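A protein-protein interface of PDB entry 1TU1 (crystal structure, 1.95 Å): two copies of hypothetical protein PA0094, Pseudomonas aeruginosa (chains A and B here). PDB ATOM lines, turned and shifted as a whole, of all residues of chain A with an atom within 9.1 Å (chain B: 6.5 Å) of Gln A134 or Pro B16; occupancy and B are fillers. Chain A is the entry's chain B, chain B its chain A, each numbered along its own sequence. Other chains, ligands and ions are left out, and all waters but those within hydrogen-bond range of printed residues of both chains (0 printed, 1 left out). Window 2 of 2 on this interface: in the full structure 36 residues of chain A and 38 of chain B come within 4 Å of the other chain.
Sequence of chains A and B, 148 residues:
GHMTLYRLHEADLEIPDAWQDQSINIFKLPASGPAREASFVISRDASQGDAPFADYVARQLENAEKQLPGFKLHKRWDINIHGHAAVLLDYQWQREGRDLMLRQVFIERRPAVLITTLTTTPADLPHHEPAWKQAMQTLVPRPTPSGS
Phe A27 touches Ile B15 (CE1 to CG2, 3.9 Å). Phe A27 touches Trp B19. Phe A27 touches Gln B20 (CA to O, 3.2 Å). NE1 of Trp B19 touches CG of Leu A29, 3.3 Å away. Pro A30 touches Ala B18 (CG to O, 3.3 Å). CZ3 of Trp B19 touches CD2 of Phe A40, at 3.5 Å. Ala A131 touches Trp B19. Gln A134 touches Pro B16 (NE2 to CG, 3.3 Å). Glu B14 touches Ala A135 (O to CA, 3.4 Å). CH2 of Trp B19 touches CB of Ala A135, 3.9 Å away.
OD2 of Asp B17 is in hydrogen-bond range of N of Met B3 (3.4 Å). O of Thr B4 sits at hydrogen-bond distance from N of Ile B15, 2.9 Å away. The backbone carbonyl oxygen (O) of Phe A27 lies within hydrogen-bond range of the backbone NH (N) of Phe A40. The backbone carbonyl oxygen (O) of Gln A134 sits at hydrogen-bond distance from the side-chain hydroxyl (OG1) of Thr A138 (3.1 Å). The backbone carbonyl oxygen (O) of Ala A135 sits at hydrogen-bond distance from the side-chain hydroxyl (OG1) of Thr A138, 2.8 Å away.
Hydrophobic or aromatic side chains of chain A within 4 Å of the printed part of chain B: Phe A27, Leu A29, Pro A30, Phe A40 and Ala A135. Hydrophobic or aromatic side chains of chain B that line the printed part of chain A: Met B3, Ile B15, Pro B16 and Trp B19. Among the printed residues, 14 pairs touch across the chains.
No position is printed for both chains. Of the 14 pairs that touch across the chains among the printed residues, none has its exchanged pair printed and touching as well.
The side-chain sulfur of Met B3 lies close to the side-chain amide nitrogen of Gln A134. N of Glu B14 lies within hydrogen-bond range of OG1 of Thr A138. The backbone carbonyl oxygen (O) of Gln B20 lies within hydrogen-bond range of the backbone NH (N) of Lys A28 (2.8 Å).
Of the printed residues of chain B, Lys A28 touches Trp B19 (3.3 Å) and Gln B20 (2.8 Å). Of the printed residues of chain B, Pro A30 touches Ala B18 (3.3 Å). Of the printed residues of chain B, Ala A131 touches Trp B19. Printed residues of chain B within 4 Å of Gln A134: Met B3 and Pro B16. Of the printed residues of chain B, Ala A135 touches Glu B14 and Trp B19. His B2 touches none of the printed residues of chain A. Ile B15 touches one residue of chain A. Pro B16 touches just one residue of chain A: Gln A134. Printed residues of chain A within 4 Å of Ala B18: Pro A30 (3.3 Å). The nearest printed residue of chain B that does not touch Ala A131 is Pro B16 (4.5 Å).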
ATOM      1  N   PHE A  27     -18.718  -9.539 -15.700  1.00  0.00           N
ATOM      2  CA  PHE A  27     -18.870  -8.483 -16.695  1.00  0.00           C
ATOM      3  C   PHE A  27     -18.234  -8.964 -18.004  1.00  0.00           C
ATOM      4  O   PHE A  27     -17.114  -9.468 -18.018  1.00  0.00           O
ATOM      5  CB  PHE A  27     -18.218  -7.185 -16.227  1.00  0.00           C
ATOM      6  CG  PHE A  27     -18.837  -6.607 -14.987  1.00  0.00           C
ATOM      7  CD1 PHE A  27     -19.937  -5.774 -15.077  1.00  0.00           C
ATOM      8  CD2 PHE A  27     -18.315  -6.887 -13.727  1.00  0.00           C
ATOM      9  CE1 PHE A  27     -20.521  -5.249 -13.936  1.00  0.00           C
ATOM     10  CE2 PHE A  27     -18.920  -6.386 -12.583  1.00  0.00           C
ATOM     11  CZ  PHE A  27     -20.008  -5.558 -12.689  1.00  0.00           C
ATOM     12  N   LYS A  28     -18.958  -8.819 -19.104  1.00  0.00           N
ATOM     13  CA  LYS A  28     -18.443  -9.129 -20.435  1.00  0.00           C
ATOM     14  C   LYS A  28     -17.926  -7.844 -21.069  1.00  0.00           C
ATOM     15  O   LYS A  28     -18.664  -6.874 -21.180  1.00  0.00           O
ATOM     16  CB  LYS A  28     -19.566  -9.711 -21.301  1.00  0.00           C
ATOM     17  CG  LYS A  28     -19.123 -10.178 -22.702  1.00  0.00           C
ATOM     18  CD  LYS A  28     -20.342 -10.515 -23.606  1.00  0.00           C
ATOM     19  CE  LYS A  28     -19.934 -10.931 -25.025  1.00  0.00           C
ATOM     20  NZ  LYS A  28     -21.034 -10.782 -26.056  1.00  0.00           N
ATOM     21  N   LEU A  29     -16.657  -7.843 -21.456  1.00  0.00           N
ATOM     22  CA  LEU A  29     -16.025  -6.717 -22.155  1.00  0.00           C
ATOM     23  C   LEU A  29     -16.239  -6.978 -23.658  1.00  0.00           C
ATOM     24  O   LEU A  29     -15.937  -8.057 -24.147  1.00  0.00           O
ATOM     25  CB  LEU A  29     -14.516  -6.639 -21.857  1.00  0.00           C
ATOM     26  CG  LEU A  29     -14.094  -6.045 -20.521  1.00  0.00           C
ATOM     27  CD1 LEU A  29     -14.511  -6.974 -19.376  1.00  0.00           C
ATOM     28  CD2 LEU A  29     -12.613  -5.769 -20.459  1.00  0.00           C
ATOM     29  N   PRO A  30     -16.806  -6.017 -24.369  1.00  0.00           N
ATOM     30  CA  PRO A  30     -17.073  -6.195 -25.798  1.00  0.00           C
ATOM     31  C   PRO A  30     -15.796  -6.316 -26.623  1.00  0.00           C
ATOM     32  O   PRO A  30     -14.795  -5.690 -26.301  1.00  0.00           O
ATOM     33  CB  PRO A  30     -17.806  -4.907 -26.203  1.00  0.00           C
ATOM     34  CG  PRO A  30     -18.093  -4.172 -24.985  1.00  0.00           C
ATOM     35  CD  PRO A  30     -17.262  -4.717 -23.870  1.00  0.00           C
ATOM     36  N   PHE A  40     -14.405  -9.941 -17.034  1.00  0.00           N
ATOM     37  CA  PHE A  40     -13.893  -9.429 -15.786  1.00  0.00           C
ATOM     38  C   PHE A  40     -14.802  -9.947 -14.679  1.00  0.00           C
ATOM     39  O   PHE A  40     -15.987  -9.580 -14.597  1.00  0.00           O
ATOM     40  CB  PHE A  40     -13.925  -7.912 -15.804  1.00  0.00           C
ATOM     41  CG  PHE A  40     -13.377  -7.260 -14.548  1.00  0.00           C
ATOM     42  CD1 PHE A  40     -12.002  -7.168 -14.337  1.00  0.00           C
ATOM     43  CD2 PHE A  40     -14.224  -6.737 -13.597  1.00  0.00           C
ATOM     44  CE1 PHE A  40     -11.502  -6.561 -13.189  1.00  0.00           C
ATOM     45  CE2 PHE A  40     -13.728  -6.128 -12.468  1.00  0.00           C
ATOM     46  CZ  PHE A  40     -12.365  -6.027 -12.265  1.00  0.00           C
ATOM     47  N   ARG A 103      -5.232 -11.904 -16.020  1.00  0.00           N
ATOM     48  CA  ARG A 103      -4.693 -10.889 -15.144  1.00  0.00           C
ATOM     49  C   ARG A 103      -5.558 -10.916 -13.899  1.00  0.00           C
ATOM     50  O   ARG A 103      -6.737 -10.543 -13.908  1.00  0.00           O
ATOM     51  CB  ARG A 103      -4.724  -9.556 -15.846  1.00  0.00           C
ATOM     52  CG  ARG A 103      -4.355  -8.390 -14.942  1.00  0.00           C
ATOM     53  CD  ARG A 103      -3.971  -7.169 -15.716  1.00  0.00           C
ATOM     54  NE  ARG A 103      -2.673  -7.298 -16.378  1.00  0.00           N
ATOM     55  CZ  ARG A 103      -2.141  -6.333 -17.101  1.00  0.00           C
ATOM     56  NH1 ARG A 103      -2.804  -5.194 -17.310  1.00  0.00           N
ATOM     57  NH2 ARG A 103      -0.964  -6.514 -17.659  1.00  0.00           N
ATOM     58  N   HIS A 128      -7.591  -4.714 -24.033  1.00  0.00           N
ATOM     59  CA  HIS A 128      -8.494  -4.578 -22.874  1.00  0.00           C
ATOM     60  C   HIS A 128      -7.878  -3.919 -21.650  1.00  0.00           C
ATOM     61  O   HIS A 128      -8.596  -3.533 -20.721  1.00  0.00           O
ATOM     62  CB  HIS A 128      -9.044  -5.941 -22.490  1.00  0.00           C
ATOM     63  CG  HIS A 128      -9.963  -6.511 -23.515  1.00  0.00           C
ATOM     64  ND1 HIS A 128     -11.130  -5.880 -23.896  1.00  0.00           N
ATOM     65  CD2 HIS A 128      -9.872  -7.628 -24.269  1.00  0.00           C
ATOM     66  CE1 HIS A 128     -11.733  -6.607 -24.820  1.00  0.00           C
ATOM     67  NE2 HIS A 128     -10.995  -7.681 -25.056  1.00  0.00           N
ATOM     68  N   GLU A 129      -6.560  -3.762 -21.658  1.00  0.00           N
ATOM     69  CA  GLU A 129      -5.853  -3.194 -20.507  1.00  0.00           C
ATOM     70  C   GLU A 129      -6.342  -1.814 -20.060  1.00  0.00           C
ATOM     71  O   GLU A 129      -6.525  -1.599 -18.881  1.00  0.00           O
ATOM     72  CB  GLU A 129      -4.347  -3.150 -20.796  1.00  0.00           C
ATOM     73  CG  GLU A 129      -3.520  -2.454 -19.736  1.00  0.00           C
ATOM     74  CD  GLU A 129      -2.059  -2.791 -19.903  1.00  0.00           C
ATOM     75  OE1 GLU A 129      -1.546  -2.607 -21.044  1.00  0.00           O
ATOM     76  OE2 GLU A 129      -1.459  -3.286 -18.929  1.00  0.00           O
ATOM     77  N   PRO A 130      -6.550  -0.868 -20.965  1.00  0.00           N
ATOM     78  CA  PRO A 130      -7.038   0.452 -20.543  1.00  0.00           C
ATOM     79  C   PRO A 130      -8.360   0.398 -19.752  1.00  0.00           C
ATOM     80  O   PRO A 130      -8.470   1.033 -18.712  1.00  0.00           O
ATOM     81  CB  PRO A 130      -7.184   1.211 -21.871  1.00  0.00           C
ATOM     82  CG  PRO A 130      -6.203   0.570 -22.753  1.00  0.00           C
ATOM     83  CD  PRO A 130      -6.327  -0.913 -22.419  1.00  0.00           C
ATOM     84  N   ALA A 131      -9.320  -0.391 -20.214  1.00  0.00           N
ATOM     85  CA  ALA A 131     -10.614  -0.494 -19.535  1.00  0.00           C
ATOM     86  C   ALA A 131     -10.453  -1.236 -18.197  1.00  0.00           C
ATOM     87  O   ALA A 131     -11.014  -0.839 -17.174  1.00  0.00           O
ATOM     88  CB  ALA A 131     -11.629  -1.182 -20.436  1.00  0.00           C
ATOM     89  N   TRP A 132      -9.653  -2.287 -18.203  1.00  0.00           N
ATOM     90  CA  TRP A 132      -9.337  -3.022 -16.978  1.00  0.00           C
ATOM     91  C   TRP A 132      -8.717  -2.096 -15.921  1.00  0.00           C
ATOM     92  O   TRP A 132      -9.121  -2.085 -14.759  1.00  0.00           O
ATOM     93  CB  TRP A 132      -8.382  -4.157 -17.288  1.00  0.00           C
ATOM     94  CG  TRP A 132      -7.855  -4.799 -16.072  1.00  0.00           C
ATOM     95  CD1 TRP A 132      -8.428  -5.829 -15.373  1.00  0.00           C
ATOM     96  CD2 TRP A 132      -6.659  -4.460 -15.376  1.00  0.00           C
ATOM     97  NE1 TRP A 132      -7.648  -6.151 -14.294  1.00  0.00           N
ATOM     98  CE2 TRP A 132      -6.558  -5.324 -14.266  1.00  0.00           C
ATOM     99  CE3 TRP A 132      -5.642  -3.512 -15.584  1.00  0.00           C
ATOM    100  CZ2 TRP A 132      -5.499  -5.267 -13.367  1.00  0.00           C
ATOM    101  CZ3 TRP A 132      -4.586  -3.456 -14.682  1.00  0.00           C
ATOM    102  CH2 TRP A 132      -4.527  -4.323 -13.586  1.00  0.00           C
ATOM    103  N   LYS A 133      -7.747  -1.308 -16.365  1.00  0.00           N
ATOM    104  CA  LYS A 133      -6.987  -0.437 -15.481  1.00  0.00           C
ATOM    105  C   LYS A 133      -7.903   0.629 -14.875  1.00  0.00           C
ATOM    106  O   LYS A 133      -7.830   0.880 -13.680  1.00  0.00           O
ATOM    107  CB  LYS A 133      -5.770   0.150 -16.221  1.00  0.00           C
ATOM    108  CG  LYS A 133      -4.537   0.419 -15.357  1.00  0.00           C
ATOM    109  CD  LYS A 133      -3.441   1.197 -16.136  1.00  0.00           C
ATOM    110  CE  LYS A 133      -2.844   0.361 -17.283  1.00  0.00           C
ATOM    111  NZ  LYS A 133      -2.008   1.148 -18.264  1.00  0.00           N
ATOM    112  N   GLN A 134      -8.800   1.210 -15.661  1.00  0.00           N
ATOM    113  CA  GLN A 134      -9.726   2.225 -15.125  1.00  0.00           C
ATOM    114  C   GLN A 134     -10.686   1.681 -14.076  1.00  0.00           C
ATOM    115  O   GLN A 134     -10.919   2.348 -13.061  1.00  0.00           O
ATOM    116  CB  GLN A 134     -10.509   2.977 -16.223  1.00  0.00           C
ATOM    117  CG  GLN A 134     -11.496   2.164 -17.047  1.00  0.00           C
ATOM    118  CD  GLN A 134     -11.920   2.888 -18.364  1.00  0.00           C
ATOM    119  OE1 GLN A 134     -11.290   3.875 -18.765  1.00  0.00           O
ATOM    120  NE2 GLN A 134     -12.970   2.383 -19.028  1.00  0.00           N
ATOM    121  N   ALA A 135     -11.206   0.477 -14.280  1.00  0.00           N
ATOM    122  CA  ALA A 135     -11.982  -0.187 -13.253  1.00  0.00           C
ATOM    123  C   ALA A 135     -11.152  -0.501 -12.001  1.00  0.00           C
ATOM    124  O   ALA A 135     -11.598  -0.256 -10.897  1.00  0.00           O
ATOM    125  CB  ALA A 135     -12.605  -1.472 -13.791  1.00  0.00           C
ATOM    126  N   MET A 136      -9.967  -1.073 -12.175  1.00  0.00           N
ATOM    127  CA  MET A 136      -9.177  -1.513 -11.014  1.00  0.00           C
ATOM    128  C   MET A 136      -8.658  -0.326 -10.188  1.00  0.00           C
ATOM    129  O   MET A 136      -8.578  -0.407  -8.957  1.00  0.00           O
ATOM    130  CB  MET A 136      -8.013  -2.401 -11.456  1.00  0.00           C
ATOM    131  CG  MET A 136      -8.384  -3.882 -11.645  1.00  0.00           C
ATOM    132  SD  MET A 136      -9.302  -4.636 -10.261  1.00  0.00           S
ATOM    133  CE  MET A 136      -8.099  -4.552  -8.945  1.00  0.00           C
ATOM    134  N   GLN A 137      -8.368   0.783 -10.857  1.00  0.00           N
ATOM    135  CA  GLN A 137      -7.875   1.998 -10.192  1.00  0.00           C
ATOM    136  C   GLN A 137      -8.947   2.703  -9.374  1.00  0.00           C
ATOM    137  O   GLN A 137      -8.636   3.564  -8.557  1.00  0.00           O
ATOM    138  CB  GLN A 137      -7.330   2.974 -11.236  1.00  0.00           C
ATOM    139  CG  GLN A 137      -6.052   2.477 -11.790  1.00  0.00           C
ATOM    140  CD  GLN A 137      -5.402   3.423 -12.752  1.00  0.00           C
ATOM    141  OE1 GLN A 137      -6.082   4.194 -13.447  1.00  0.00           O
ATOM    142  NE2 GLN A 137      -4.086   3.330 -12.846  1.00  0.00           N
ATOM    143  N   THR A 138     -10.204   2.330  -9.578  1.00  0.00           N
ATOM    144  CA  THR A 138     -11.295   2.944  -8.851  1.00  0.00           C
ATOM    145  C   THR A 138     -11.914   1.998  -7.836  1.00  0.00           C
ATOM    146  O   THR A 138     -12.902   2.332  -7.197  1.00  0.00           O
ATOM    147  CB  THR A 138     -12.380   3.414  -9.851  1.00  0.00           C
ATOM    148  OG1 THR A 138     -12.818   2.302 -10.641  1.00  0.00           O
ATOM    149  CG2 THR A 138     -11.797   4.401 -10.888  1.00  0.00           C
ATOM    150  N   LEU A 139     -11.373   0.799  -7.707  1.00  0.00           N
ATOM    151  CA  LEU A 139     -11.904  -0.176  -6.766  1.00  0.00           C
ATOM    152  C   LEU A 139     -11.512   0.238  -5.363  1.00  0.00           C
ATOM    153  O   LEU A 139     -10.319   0.261  -5.024  1.00  0.00           O
ATOM    154  CB  LEU A 139     -11.357  -1.572  -7.068  1.00  0.00           C
ATOM    155  CG  LEU A 139     -11.992  -2.753  -6.328  1.00  0.00           C
ATOM    156  CD1 LEU A 139     -11.663  -4.023  -7.065  1.00  0.00           C
ATOM    157  CD2 LEU A 139     -11.531  -2.861  -4.881  1.00  0.00           C
ATOM    158  N   VAL A 140     -12.510   0.538  -4.548  1.00  0.00           N
ATOM    159  CA  VAL A 140     -12.320   0.872  -3.141  1.00  0.00           C
ATOM    160  C   VAL A 140     -12.958  -0.184  -2.232  1.00  0.00           C
ATOM    161  O   VAL A 140     -14.178  -0.284  -2.145  1.00  0.00           O
ATOM    162  CB  VAL A 140     -12.945   2.259  -2.828  1.00  0.00           C
ATOM    163  CG1 VAL A 140     -12.745   2.623  -1.336  1.00  0.00           C
ATOM    164  CG2 VAL A 140     -12.334   3.338  -3.743  1.00  0.00           C
ATOM    165  N   GLY B   1     -14.479   8.698 -18.187  1.00  0.00           N
ATOM    166  CA  GLY B   1     -15.198   8.898 -19.493  1.00  0.00           C
ATOM    167  C   GLY B   1     -16.648   8.409 -19.510  1.00  0.00           C
ATOM    168  O   GLY B   1     -17.560   9.145 -19.117  1.00  0.00           O
ATOM    169  N   HIS B   2     -16.862   7.182 -19.988  1.00  0.00           N
ATOM    170  CA  HIS B   2     -18.188   6.552 -20.029  1.00  0.00           C
ATOM    171  C   HIS B   2     -18.234   5.381 -19.032  1.00  0.00           C
ATOM    172  O   HIS B   2     -18.038   4.227 -19.414  1.00  0.00           O
ATOM    173  CB  HIS B   2     -18.494   6.007 -21.434  1.00  0.00           C
ATOM    174  CG  HIS B   2     -18.780   7.059 -22.466  1.00  0.00           C
ATOM    175  ND1 HIS B   2     -18.931   6.758 -23.805  1.00  0.00           N
ATOM    176  CD2 HIS B   2     -18.941   8.402 -22.360  1.00  0.00           C
ATOM    177  CE1 HIS B   2     -19.172   7.869 -24.479  1.00  0.00           C
ATOM    178  NE2 HIS B   2     -19.182   8.881 -23.626  1.00  0.00           N
ATOM    179  N   MET B   3     -18.467   5.680 -17.756  1.00  0.00           N
ATOM    180  CA  MET B   3     -18.554   4.639 -16.725  1.00  0.00           C
ATOM    181  C   MET B   3     -19.591   4.973 -15.650  1.00  0.00           C
ATOM    182  O   MET B   3     -20.126   6.072 -15.603  1.00  0.00           O
ATOM    183  CB  MET B   3     -17.186   4.466 -16.053  1.00  0.00           C
ATOM    184  CG  MET B   3     -16.041   4.175 -17.005  1.00  0.00           C
ATOM    185  SD  MET B   3     -14.461   4.275 -16.223  1.00  0.00           S
ATOM    186  CE  MET B   3     -14.442   2.666 -15.333  1.00  0.00           C
ATOM    187  N   THR B   4     -19.866   4.001 -14.790  1.00  0.00           N
ATOM    188  CA  THR B   4     -20.794   4.168 -13.687  1.00  0.00           C
ATOM    189  C   THR B   4     -20.316   3.445 -12.413  1.00  0.00           C
ATOM    190  O   THR B   4     -19.760   2.365 -12.485  1.00  0.00           O
ATOM    191  CB  THR B   4     -22.142   3.655 -14.134  1.00  0.00           C
ATOM    192  OG1 THR B   4     -22.584   4.440 -15.261  1.00  0.00           O
ATOM    193  CG2 THR B   4     -23.216   3.882 -13.066  1.00  0.00           C
ATOM    194  N   GLU B  14     -15.757   1.750 -10.442  1.00  0.00           N
ATOM    195  CA  GLU B  14     -16.387   2.264 -11.654  1.00  0.00           C
ATOM    196  C   GLU B  14     -16.307   1.224 -12.732  1.00  0.00           C
ATOM    197  O   GLU B  14     -15.223   0.728 -13.027  1.00  0.00           O
ATOM    198  CB  GLU B  14     -15.707   3.554 -12.127  1.00  0.00           C
ATOM    199  CG  GLU B  14     -15.891   4.669 -11.120  1.00  0.00           C
ATOM    200  CD  GLU B  14     -15.312   5.996 -11.574  1.00  0.00           C
ATOM    201  OE1 GLU B  14     -14.636   6.064 -12.636  1.00  0.00           O
ATOM    202  OE2 GLU B  14     -15.506   6.950 -10.826  1.00  0.00           O
ATOM    203  N   ILE B  15     -17.455   0.894 -13.319  1.00  0.00           N
ATOM    204  CA  ILE B  15     -17.550  -0.064 -14.404  1.00  0.00           C
ATOM    205  C   ILE B  15     -17.903   0.636 -15.750  1.00  0.00           C
ATOM    206  O   ILE B  15     -18.897   1.340 -15.810  1.00  0.00           O
ATOM    207  CB  ILE B  15     -18.618  -1.109 -14.045  1.00  0.00           C
ATOM    208  CG1 ILE B  15     -18.138  -1.992 -12.847  1.00  0.00           C
ATOM    209  CG2 ILE B  15     -18.984  -1.972 -15.272  1.00  0.00           C
ATOM    210  CD1 ILE B  15     -16.958  -2.906 -13.180  1.00  0.00           C
ATOM    211  N   PRO B  16     -17.125   0.418 -16.812  1.00  0.00           N
ATOM    212  CA  PRO B  16     -17.465   0.973 -18.131  1.00  0.00           C
ATOM    213  C   PRO B  16     -18.872   0.574 -18.571  1.00  0.00           C
ATOM    214  O   PRO B  16     -19.249  -0.575 -18.436  1.00  0.00           O
ATOM    215  CB  PRO B  16     -16.393   0.388 -19.047  1.00  0.00           C
ATOM    216  CG  PRO B  16     -15.263   0.122 -18.176  1.00  0.00           C
ATOM    217  CD  PRO B  16     -15.858  -0.320 -16.855  1.00  0.00           C
ATOM    218  N   ASP B  17     -19.656   1.538 -19.058  1.00  0.00           N
ATOM    219  CA  ASP B  17     -21.044   1.292 -19.491  1.00  0.00           C
ATOM    220  C   ASP B  17     -21.139   0.267 -20.618  1.00  0.00           C
ATOM    221  O   ASP B  17     -22.141  -0.399 -20.763  1.00  0.00           O
ATOM    222  CB  ASP B  17     -21.723   2.600 -19.947  1.00  0.00           C
ATOM    223  CG  ASP B  17     -21.617   3.707 -18.916  1.00  0.00           C
ATOM    224  OD1 ASP B  17     -21.754   3.402 -17.706  1.00  0.00           O
ATOM    225  OD2 ASP B  17     -21.399   4.903 -19.217  1.00  0.00           O
ATOM    226  N   ALA B  18     -20.084   0.134 -21.402  1.00  0.00           N
ATOM    227  CA  ALA B  18     -20.065  -0.842 -22.477  1.00  0.00           C
ATOM    228  C   ALA B  18     -19.994  -2.285 -21.971  1.00  0.00           C
ATOM    229  O   ALA B  18     -20.313  -3.200 -22.716  1.00  0.00           O
ATOM    230  CB  ALA B  18     -18.910  -0.566 -23.396  1.00  0.00           C
ATOM    231  N   TRP B  19     -19.549  -2.497 -20.726  1.00  0.00           N
ATOM    232  CA  TRP B  19     -19.495  -3.855 -20.156  1.00  0.00           C
ATOM    233  C   TRP B  19     -20.894  -4.405 -19.877  1.00  0.00           C
ATOM    234  O   TRP B  19     -21.756  -3.687 -19.381  1.00  0.00           O
ATOM    235  CB  TRP B  19     -18.693  -3.876 -18.847  1.00  0.00           C
ATOM    236  CG  TRP B  19     -17.219  -3.604 -19.009  1.00  0.00           C
ATOM    237  CD1 TRP B  19     -16.571  -3.151 -20.122  1.00  0.00           C
ATOM    238  CD2 TRP B  19     -16.204  -3.784 -18.005  1.00  0.00           C
ATOM    239  NE1 TRP B  19     -15.222  -3.042 -19.873  1.00  0.00           N
ATOM    240  CE2 TRP B  19     -14.967  -3.405 -18.579  1.00  0.00           C
ATOM    241  CE3 TRP B  19     -16.218  -4.211 -16.679  1.00  0.00           C
ATOM    242  CZ2 TRP B  19     -13.758  -3.461 -17.882  1.00  0.00           C
ATOM    243  CZ3 TRP B  19     -14.987  -4.249 -15.969  1.00  0.00           C
ATOM    244  CH2 TRP B  19     -13.789  -3.878 -16.587  1.00  0.00           C
ATOM    245  N   GLN B  20     -21.089  -5.691 -20.138  1.00  0.00           N
ATOM    246  CA  GLN B  20     -22.376  -6.330 -19.937  1.00  0.00           C
ATOM    247  C   GLN B  20     -22.362  -7.101 -18.614  1.00  0.00           C
ATOM    248  O   GLN B  20     -21.551  -7.979 -18.415  1.00  0.00           O
ATOM    249  CB  GLN B  20     -22.666  -7.277 -21.101  1.00  0.00           C
ATOM    250  CG  GLN B  20     -23.898  -8.130 -20.942  1.00  0.00           C
ATOM    251  CD  GLN B  20     -24.025  -9.168 -22.033  1.00  0.00           C
ATOM    252  OE1 GLN B  20     -23.753  -8.878 -23.199  1.00  0.00           O
ATOM    253  NE2 GLN B  20     -24.434 -10.376 -21.666  1.00  0.00           N
